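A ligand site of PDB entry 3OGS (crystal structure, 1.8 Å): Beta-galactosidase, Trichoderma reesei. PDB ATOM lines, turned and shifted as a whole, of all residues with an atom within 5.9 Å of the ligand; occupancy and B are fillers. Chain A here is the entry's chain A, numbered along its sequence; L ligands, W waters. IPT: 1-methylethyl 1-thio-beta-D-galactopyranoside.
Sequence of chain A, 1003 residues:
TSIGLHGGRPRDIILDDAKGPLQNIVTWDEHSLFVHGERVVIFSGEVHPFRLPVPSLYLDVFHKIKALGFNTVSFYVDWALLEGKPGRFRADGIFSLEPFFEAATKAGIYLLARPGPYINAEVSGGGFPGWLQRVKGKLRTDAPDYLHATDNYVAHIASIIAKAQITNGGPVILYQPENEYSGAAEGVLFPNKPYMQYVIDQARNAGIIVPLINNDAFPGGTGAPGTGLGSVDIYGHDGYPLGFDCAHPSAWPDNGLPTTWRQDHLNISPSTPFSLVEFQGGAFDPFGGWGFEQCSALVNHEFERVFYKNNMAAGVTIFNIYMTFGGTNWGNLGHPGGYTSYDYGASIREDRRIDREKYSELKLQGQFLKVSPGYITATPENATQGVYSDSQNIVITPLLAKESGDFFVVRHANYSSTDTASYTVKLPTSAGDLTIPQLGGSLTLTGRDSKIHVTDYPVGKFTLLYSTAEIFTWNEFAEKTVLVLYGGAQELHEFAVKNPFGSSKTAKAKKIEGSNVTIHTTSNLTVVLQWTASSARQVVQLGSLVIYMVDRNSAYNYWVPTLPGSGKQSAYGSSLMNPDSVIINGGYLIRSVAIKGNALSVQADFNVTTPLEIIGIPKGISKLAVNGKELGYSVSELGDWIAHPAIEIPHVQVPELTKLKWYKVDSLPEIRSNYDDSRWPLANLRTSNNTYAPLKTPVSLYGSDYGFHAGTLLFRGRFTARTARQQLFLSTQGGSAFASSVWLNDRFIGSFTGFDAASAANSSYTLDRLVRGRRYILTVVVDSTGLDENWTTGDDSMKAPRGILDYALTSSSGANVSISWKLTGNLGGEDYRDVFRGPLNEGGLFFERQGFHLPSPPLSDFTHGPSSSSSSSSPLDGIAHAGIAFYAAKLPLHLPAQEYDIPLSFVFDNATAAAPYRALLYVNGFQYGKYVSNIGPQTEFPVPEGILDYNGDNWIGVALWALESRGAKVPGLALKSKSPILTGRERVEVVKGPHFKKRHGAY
OE2 of Glu 122 sits at hydrogen-bond distance from O4 of the ligand (2.6 Å).
O6 of the ligand is in hydrogen-bond range of OH of Tyr 344, 2.7 Å away.
The side-chain carboxylate (OE2) of Glu 278 is in hydrogen-bond range of an oxygen (O2) of the ligand, at 2.8 Å.
An oxygen (O3) of the ligand sits at hydrogen-bond distance from the side-chain hydroxyl of Tyr 76 (2.8 Å).
The side-chain amide nitrogen (ND2) of Asn 120 sits at hydrogen-bond distance from an oxygen (O4) of the ligand, 2.9 Å away.
An oxygen (O2) of the ligand lies within hydrogen-bond range of the side-chain amide nitrogen (ND2) of Asn 179, 2.9 Å away.
The backbone NH of Ala 121 sits at hydrogen-bond distance from an oxygen (O3) of the ligand (3.0 Å).
The backbone carbonyl oxygen (O) of Ile 119 is in hydrogen-bond range of an oxygen (O3) of the ligand, 3.2 Å away.
The side-chain carboxylate (OE1) of Glu 122 lies within hydrogen-bond range of the side-chain hydroxyl (OH) of Tyr 342 (2.7 Å).
N of Glu 122 lies within hydrogen-bond range of OE2 of Glu 789 (3.0 Å).
The side-chain carboxylate of Glu 278 sits at hydrogen-bond distance from the side-chain hydroxyl of Tyr 240 (2.7 Å).
The side-chain carboxylate (OE2) of Glu 278 lies within hydrogen-bond range of the side-chain amide nitrogen (ND2) of Asn 215, 3.0 Å away.
The side-chain hydroxyl (OH) of Tyr 76 lies within hydrogen-bond range of the backbone carbonyl oxygen (O) of Ile 119, at 3.3 Å.
OH of Tyr 76 lies close to NH2 of Arg 114 (3.2 Å).
The backbone carbonyl oxygen (O) of Ile 119 lies within hydrogen-bond range of the side-chain amide nitrogen (ND2) of Asn 179 (3.3 Å).
O of Asp 216 sits at hydrogen-bond distance from N of Asp 238, 3.0 Å away.
Water W1 lies within hydrogen-bond range of an oxygen (O5) of the ligand and the side-chain amide nitrogen (ND2) of Asn 120.
Residues that only touch the ligand: Glu 180 (3.9 Å), Asn 215 (3.9 Å), Asp 238 (3.6 Å), Tyr 240 (3.7 Å), Phe 244 (3.96 Å), Phe 284 (3.6 Å) and Tyr 322 (3.5 Å).
Hydrophobic or aromatic side chains within 4 Å of the ligand: Tyr 76, Tyr 240, Phe 244, Phe 284, Tyr 322 and Tyr 344.
15 residues have an atom within 4 Å of the ligand: Tyr 76, Ile 119, Asn 120, Ala 121, Glu 122, Asn 179, Glu 180, Asn 215, Asp 238, Tyr 240, Phe 244, Glu 278, Phe 284, Tyr 322 and Tyr 344.
The nearest printed residue that does not touch the ligand is Tyr 342 (4.02 Å).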
ATOM      1  N   TYR A  76       5.222  23.220  32.594  1.00  0.00           N
ATOM      2  CA  TYR A  76       4.321  24.376  32.246  1.00  0.00           C
ATOM      3  C   TYR A  76       4.009  25.243  33.513  1.00  0.00           C
ATOM      4  O   TYR A  76       4.026  24.704  34.665  1.00  0.00           O
ATOM      5  CB  TYR A  76       2.955  23.931  31.599  1.00  0.00           C
ATOM      6  CG  TYR A  76       3.055  23.455  30.124  1.00  0.00           C
ATOM      7  CD1 TYR A  76       3.743  24.238  29.120  1.00  0.00           C
ATOM      8  CD2 TYR A  76       2.401  22.294  29.721  1.00  0.00           C
ATOM      9  CE1 TYR A  76       3.745  23.786  27.710  1.00  0.00           C
ATOM     10  CE2 TYR A  76       2.385  21.854  28.358  1.00  0.00           C
ATOM     11  CZ  TYR A  76       3.078  22.599  27.368  1.00  0.00           C
ATOM     12  OH  TYR A  76       3.050  22.121  26.046  1.00  0.00           O
ATOM     13  N   ARG A 114       8.535  26.409  30.777  1.00  0.00           N
ATOM     14  CA  ARG A 114       7.559  26.693  29.622  1.00  0.00           C
ATOM     15  C   ARG A 114       6.304  27.447  30.057  1.00  0.00           C
ATOM     16  O   ARG A 114       5.229  26.803  30.325  1.00  0.00           O
ATOM     17  CB  ARG A 114       7.256  25.382  28.877  1.00  0.00           C
ATOM     18  CG  ARG A 114       8.484  24.381  28.949  1.00  0.00           C
ATOM     19  CD  ARG A 114       8.332  23.334  27.761  1.00  0.00           C
ATOM     20  NE  ARG A 114       7.244  22.335  28.004  1.00  0.00           N
ATOM     21  CZ  ARG A 114       6.549  21.697  27.021  1.00  0.00           C
ATOM     22  NH1 ARG A 114       6.657  22.064  25.736  1.00  0.00           N
ATOM     23  NH2 ARG A 114       5.609  20.803  27.353  1.00  0.00           N
ATOM     24  N   ILE A 119      -0.354  27.520  26.605  1.00  0.00           N
ATOM     25  CA  ILE A 119       0.357  26.207  26.938  1.00  0.00           C
ATOM     26  C   ILE A 119      -0.328  24.928  26.314  1.00  0.00           C
ATOM     27  O   ILE A 119       0.312  23.897  26.149  1.00  0.00           O
ATOM     28  CB  ILE A 119       0.630  25.963  28.494  1.00  0.00           C
ATOM     29  CG1 ILE A 119      -0.704  25.855  29.347  1.00  0.00           C
ATOM     30  CG2 ILE A 119       1.649  27.036  29.002  1.00  0.00           C
ATOM     31  CD1 ILE A 119      -0.405  25.294  30.802  1.00  0.00           C
ATOM     32  N   ASN A 120      -1.595  25.058  25.874  1.00  0.00           N
ATOM     33  CA  ASN A 120      -2.474  23.910  25.392  1.00  0.00           C
ATOM     34  C   ASN A 120      -2.635  22.903  26.613  1.00  0.00           C
ATOM     35  O   ASN A 120      -3.423  23.213  27.484  1.00  0.00           O
ATOM     36  CB  ASN A 120      -1.922  23.274  24.041  1.00  0.00           C
ATOM     37  CG  ASN A 120      -2.993  22.586  23.202  1.00  0.00           C
ATOM     38  OD1 ASN A 120      -3.950  23.279  22.757  1.00  0.00           O
ATOM     39  ND2 ASN A 120      -2.879  21.263  22.956  1.00  0.00           N
ATOM     40  N   ALA A 121      -1.855  21.797  26.701  1.00  0.00           N
ATOM     41  CA  ALA A 121      -1.708  20.970  27.953  1.00  0.00           C
ATOM     42  C   ALA A 121      -2.949  20.255  28.476  1.00  0.00           C
ATOM     43  O   ALA A 121      -2.905  19.658  29.584  1.00  0.00           O
ATOM     44  CB  ALA A 121      -1.092  21.860  29.132  1.00  0.00           C
ATOM     45  N   GLU A 122      -4.002  20.175  27.633  1.00  0.00           N
ATOM     46  CA  GLU A 122      -5.296  19.653  28.099  1.00  0.00           C
ATOM     47  C   GLU A 122      -5.812  20.356  29.366  1.00  0.00           C
ATOM     48  O   GLU A 122      -6.521  19.739  30.180  1.00  0.00           O
ATOM     49  CB  GLU A 122      -5.238  18.082  28.276  1.00  0.00           C
ATOM     50  CG  GLU A 122      -5.149  17.265  26.852  1.00  0.00           C
ATOM     51  CD  GLU A 122      -3.733  17.363  26.190  1.00  0.00           C
ATOM     52  OE1 GLU A 122      -2.789  16.901  26.862  1.00  0.00           O
ATOM     53  OE2 GLU A 122      -3.591  17.886  25.031  1.00  0.00           O
ATOM     54  N   ASN A 179       3.786  28.115  22.445  1.00  0.00           N
ATOM     55  CA  ASN A 179       3.678  26.618  22.418  1.00  0.00           C
ATOM     56  C   ASN A 179       3.150  26.107  21.041  1.00  0.00           C
ATOM     57  O   ASN A 179       2.011  26.440  20.605  1.00  0.00           O
ATOM     58  CB  ASN A 179       2.723  26.091  23.583  1.00  0.00           C
ATOM     59  CG  ASN A 179       2.768  24.547  23.714  1.00  0.00           C
ATOM     60  OD1 ASN A 179       3.731  24.008  24.259  1.00  0.00           O
ATOM     61  ND2 ASN A 179       1.721  23.822  23.147  1.00  0.00           N
ATOM     62  N   GLU A 180       3.931  25.260  20.391  1.00  0.00           N
ATOM     63  CA  GLU A 180       3.472  24.587  19.167  1.00  0.00           C
ATOM     64  C   GLU A 180       2.839  25.590  18.133  1.00  0.00           C
ATOM     65  O   GLU A 180       1.703  25.386  17.593  1.00  0.00           O
ATOM     66  CB  GLU A 180       2.539  23.397  19.572  1.00  0.00           C
ATOM     67  CG  GLU A 180       2.165  22.458  18.372  1.00  0.00           C
ATOM     68  CD  GLU A 180       0.720  22.626  17.964  1.00  0.00           C
ATOM     69  OE1 GLU A 180      -0.126  23.032  18.821  1.00  0.00           O
ATOM     70  OE2 GLU A 180       0.435  22.348  16.769  1.00  0.00           O
ATOM     71  N   ASN A 215       8.983  24.291  20.012  1.00  0.00           N
ATOM     72  CA  ASN A 215       8.427  22.927  19.988  1.00  0.00           C
ATOM     73  C   ASN A 215       7.401  22.823  18.831  1.00  0.00           C
ATOM     74  O   ASN A 215       6.232  22.624  19.032  1.00  0.00           O
ATOM     75  CB  ASN A 215       7.824  22.476  21.364  1.00  0.00           C
ATOM     76  CG  ASN A 215       6.597  23.320  21.791  1.00  0.00           C
ATOM     77  OD1 ASN A 215       6.510  24.507  21.475  1.00  0.00           O
ATOM     78  ND2 ASN A 215       5.601  22.661  22.453  1.00  0.00           N
ATOM     79  N   ASP A 216       7.891  23.010  17.616  1.00  0.00           N
ATOM     80  CA  ASP A 216       7.077  22.821  16.339  1.00  0.00           C
ATOM     81  C   ASP A 216       6.373  21.396  16.293  1.00  0.00           C
ATOM     82  O   ASP A 216       6.982  20.395  16.680  1.00  0.00           O
ATOM     83  CB  ASP A 216       8.065  23.028  15.161  1.00  0.00           C
ATOM     84  CG  ASP A 216       7.426  23.607  13.840  1.00  0.00           C
ATOM     85  OD1 ASP A 216       6.178  23.828  13.758  1.00  0.00           O
ATOM     86  OD2 ASP A 216       8.202  23.846  12.813  1.00  0.00           O
ATOM     87  N   ALA A 217       5.111  21.318  15.836  1.00  0.00           N
ATOM     88  CA  ALA A 217       4.302  20.067  15.786  1.00  0.00           C
ATOM     89  C   ALA A 217       4.922  18.986  14.912  1.00  0.00           C
ATOM     90  O   ALA A 217       4.772  17.765  15.214  1.00  0.00           O
ATOM     91  CB  ALA A 217       2.851  20.350  15.311  1.00  0.00           C
ATOM     92  N   ASP A 238       8.336  18.011  17.843  1.00  0.00           N
ATOM     93  CA  ASP A 238       7.588  17.041  18.723  1.00  0.00           C
ATOM     94  C   ASP A 238       7.371  15.723  17.984  1.00  0.00           C
ATOM     95  O   ASP A 238       7.630  15.635  16.705  1.00  0.00           O
ATOM     96  CB  ASP A 238       6.210  17.642  19.152  1.00  0.00           C
ATOM     97  CG  ASP A 238       6.319  19.052  19.706  1.00  0.00           C
ATOM     98  OD1 ASP A 238       7.347  19.348  20.363  1.00  0.00           O
ATOM     99  OD2 ASP A 238       5.381  19.892  19.421  1.00  0.00           O
ATOM    100  N   GLY A 239       6.895  14.684  18.702  1.00  0.00           N
ATOM    101  CA  GLY A 239       6.477  13.478  17.946  1.00  0.00           C
ATOM    102  C   GLY A 239       5.513  12.634  18.763  1.00  0.00           C
ATOM    103  O   GLY A 239       5.855  12.261  19.917  1.00  0.00           O
ATOM    104  N   TYR A 240       4.353  12.286  18.185  1.00  0.00           N
ATOM    105  CA  TYR A 240       3.416  11.352  18.851  1.00  0.00           C
ATOM    106  C   TYR A 240       2.959  10.344  17.813  1.00  0.00           C
ATOM    107  O   TYR A 240       1.815  10.400  17.352  1.00  0.00           O
ATOM    108  CB  TYR A 240       2.201  12.123  19.423  1.00  0.00           C
ATOM    109  CG  TYR A 240       2.559  13.087  20.612  1.00  0.00           C
ATOM    110  CD1 TYR A 240       3.073  14.388  20.390  1.00  0.00           C
ATOM    111  CD2 TYR A 240       2.382  12.668  21.946  1.00  0.00           C
ATOM    112  CE1 TYR A 240       3.432  15.298  21.551  1.00  0.00           C
ATOM    113  CE2 TYR A 240       2.663  13.572  23.079  1.00  0.00           C
ATOM    114  CZ  TYR A 240       3.225  14.830  22.844  1.00  0.00           C
ATOM    115  OH  TYR A 240       3.454  15.657  23.960  1.00  0.00           O
ATOM    116  N   PHE A 244      -3.462   9.383  19.733  1.00  0.00           N
ATOM    117  CA  PHE A 244      -4.122   9.459  21.035  1.00  0.00           C
ATOM    118  C   PHE A 244      -5.333   8.578  21.366  1.00  0.00           C
ATOM    119  O   PHE A 244      -5.879   8.658  22.507  1.00  0.00           O
ATOM    120  CB  PHE A 244      -4.441  10.944  21.343  1.00  0.00           C
ATOM    121  CG  PHE A 244      -3.256  11.827  21.255  1.00  0.00           C
ATOM    122  CD1 PHE A 244      -3.052  12.674  20.128  1.00  0.00           C
ATOM    123  CD2 PHE A 244      -2.309  11.844  22.318  1.00  0.00           C
ATOM    124  CE1 PHE A 244      -1.918  13.527  20.057  1.00  0.00           C
ATOM    125  CE2 PHE A 244      -1.147  12.676  22.200  1.00  0.00           C
ATOM    126  CZ  PHE A 244      -0.989  13.499  21.097  1.00  0.00           C
ATOM    127  N   GLU A 278       9.060  17.468  22.938  1.00  0.00           N
ATOM    128  CA  GLU A 278       7.934  16.637  23.512  1.00  0.00           C
ATOM    129  C   GLU A 278       7.910  15.378  22.675  1.00  0.00           C
ATOM    130  O   GLU A 278       7.646  15.430  21.446  1.00  0.00           O
ATOM    131  CB  GLU A 278       6.573  17.258  23.340  1.00  0.00           C
ATOM    132  CG  GLU A 278       6.261  18.473  24.195  1.00  0.00           C
ATOM    133  CD  GLU A 278       4.876  19.053  23.896  1.00  0.00           C
ATOM    134  OE1 GLU A 278       3.921  18.318  23.573  1.00  0.00           O
ATOM    135  OE2 GLU A 278       4.693  20.290  24.025  1.00  0.00           O
ATOM    136  N   PHE A 284      -3.495  11.251  26.289  1.00  0.00           N
ATOM    137  CA  PHE A 284      -4.616  11.845  27.056  1.00  0.00           C
ATOM    138  C   PHE A 284      -5.817  10.908  26.767  1.00  0.00           C
ATOM    139  O   PHE A 284      -5.714   9.952  25.861  1.00  0.00           O
ATOM    140  CB  PHE A 284      -4.883  13.348  26.649  1.00  0.00           C
ATOM    141  CG  PHE A 284      -5.114  13.610  25.139  1.00  0.00           C
ATOM    142  CD1 PHE A 284      -6.305  13.214  24.520  1.00  0.00           C
ATOM    143  CD2 PHE A 284      -4.154  14.291  24.378  1.00  0.00           C
ATOM    144  CE1 PHE A 284      -6.569  13.469  23.053  1.00  0.00           C
ATOM    145  CE2 PHE A 284      -4.381  14.570  22.985  1.00  0.00           C
ATOM    146  CZ  PHE A 284      -5.584  14.159  22.312  1.00  0.00           C
ATOM    147  N   TYR A 322       6.970  13.402  27.399  1.00  0.00           N
ATOM    148  CA  TYR A 322       5.683  14.072  27.794  1.00  0.00           C
ATOM    149  C   TYR A 322       4.556  12.990  27.910  1.00  0.00           C
ATOM    150  O   TYR A 322       4.285  12.359  26.849  1.00  0.00           O
ATOM    151  CB  TYR A 322       5.265  15.150  26.753  1.00  0.00           C
ATOM    152  CG  TYR A 322       4.038  15.983  27.144  1.00  0.00           C
ATOM    153  CD1 TYR A 322       2.763  15.394  27.234  1.00  0.00           C
ATOM    154  CD2 TYR A 322       4.163  17.367  27.499  1.00  0.00           C
ATOM    155  CE1 TYR A 322       1.603  16.131  27.691  1.00  0.00           C
ATOM    156  CE2 TYR A 322       3.002  18.114  27.934  1.00  0.00           C
ATOM    157  CZ  TYR A 322       1.723  17.486  28.061  1.00  0.00           C
ATOM    158  OH  TYR A 322       0.603  18.216  28.526  1.00  0.00           O
ATOM    159  N   TYR A 342      -5.246  12.831  35.346  1.00  0.00           N
ATOM    160  CA  TYR A 342      -4.239  13.039  34.274  1.00  0.00           C
ATOM    161  C   TYR A 342      -3.077  11.980  34.457  1.00  0.00           C
ATOM    162  O   TYR A 342      -1.952  12.281  34.169  1.00  0.00           O
ATOM    163  CB  TYR A 342      -3.664  14.507  34.238  1.00  0.00           C
ATOM    164  CG  TYR A 342      -3.060  15.005  32.895  1.00  0.00           C
ATOM    165  CD1 TYR A 342      -3.803  14.936  31.674  1.00  0.00           C
ATOM    166  CD2 TYR A 342      -1.720  15.517  32.826  1.00  0.00           C
ATOM    167  CE1 TYR A 342      -3.284  15.474  30.416  1.00  0.00           C
ATOM    168  CE2 TYR A 342      -1.184  16.032  31.637  1.00  0.00           C
ATOM    169  CZ  TYR A 342      -1.975  15.994  30.392  1.00  0.00           C
ATOM    170  OH  TYR A 342      -1.469  16.506  29.212  1.00  0.00           O
ATOM    171  N   TYR A 344      -2.208   9.730  32.431  1.00  0.00           N
ATOM    172  CA  TYR A 344      -1.579   9.719  31.110  1.00  0.00           C
ATOM    173  C   TYR A 344      -1.029   8.326  30.663  1.00  0.00           C
ATOM    174  O   TYR A 344      -0.444   8.216  29.551  1.00  0.00           O
ATOM    175  CB  TYR A 344      -0.435  10.809  31.019  1.00  0.00           C
ATOM    176  CG  TYR A 344      -0.279  11.472  29.652  1.00  0.00           C
ATOM    177  CD1 TYR A 344      -1.152  12.540  29.211  1.00  0.00           C
ATOM    178  CD2 TYR A 344       0.820  11.121  28.794  1.00  0.00           C
ATOM    179  CE1 TYR A 344      -0.985  13.150  27.928  1.00  0.00           C
ATOM    180  CE2 TYR A 344       0.994  11.739  27.483  1.00  0.00           C
ATOM    181  CZ  TYR A 344       0.077  12.719  27.061  1.00  0.00           C
ATOM    182  OH  TYR A 344       0.291  13.285  25.783  1.00  0.00           O
ATOM    183  N   GLU A 789      -9.613  24.574  24.230  1.00  0.00           N
ATOM    184  CA  GLU A 789      -8.291  25.018  23.782  1.00  0.00           C
ATOM    185  C   GLU A 789      -8.376  25.890  22.491  1.00  0.00           C
ATOM    186  O   GLU A 789      -9.480  26.108  21.920  1.00  0.00           O
ATOM    187  CB  GLU A 789      -7.393  23.743  23.498  1.00  0.00           C
ATOM    188  CG  GLU A 789      -6.974  22.948  24.801  1.00  0.00           C
ATOM    189  CD  GLU A 789      -6.270  21.658  24.473  1.00  0.00           C
ATOM    190  OE1 GLU A 789      -6.625  20.934  23.461  1.00  0.00           O
ATOM    191  OE2 GLU A 789      -5.326  21.310  25.225  1.00  0.00           O
HETATM  192  C1  IPT L   1       1.166  18.875  22.122  1.00  0.00           C
HETATM  193  C2  IPT L   1       0.991  20.114  23.041  1.00  0.00           C
HETATM  194  O2  IPT L   1       2.192  20.937  22.949  1.00  0.00           O
HETATM  195  C3  IPT L   1       0.916  19.708  24.517  1.00  0.00           C
HETATM  196  O3  IPT L   1       0.629  20.865  25.346  1.00  0.00           O
HETATM  197  C4  IPT L   1      -0.172  18.620  24.793  1.00  0.00           C
HETATM  198  O4  IPT L   1      -1.449  19.244  24.453  1.00  0.00           O
HETATM  199  C5  IPT L   1       0.136  17.378  23.842  1.00  0.00           C
HETATM  200  O5  IPT L   1       0.180  17.913  22.485  1.00  0.00           O
HETATM  201  C6  IPT L   1      -0.898  16.232  23.965  1.00  0.00           C
HETATM  202  O6  IPT L   1      -0.977  15.675  25.306  1.00  0.00           O
HETATM  203  S1  IPT L   1       0.857  19.411  20.426  1.00  0.00           S
HETATM  204  C1' IPT L   1       1.282  17.820  19.715  1.00  0.00           C
HETATM  205  C2' IPT L   1       0.168  16.944  19.101  1.00  0.00           C
HETATM  206  C3' IPT L   1       2.387  17.994  18.694  1.00  0.00           C
HETATM  207  O   HOH W   1      -2.717  18.396  21.065  1.00  0.00           O
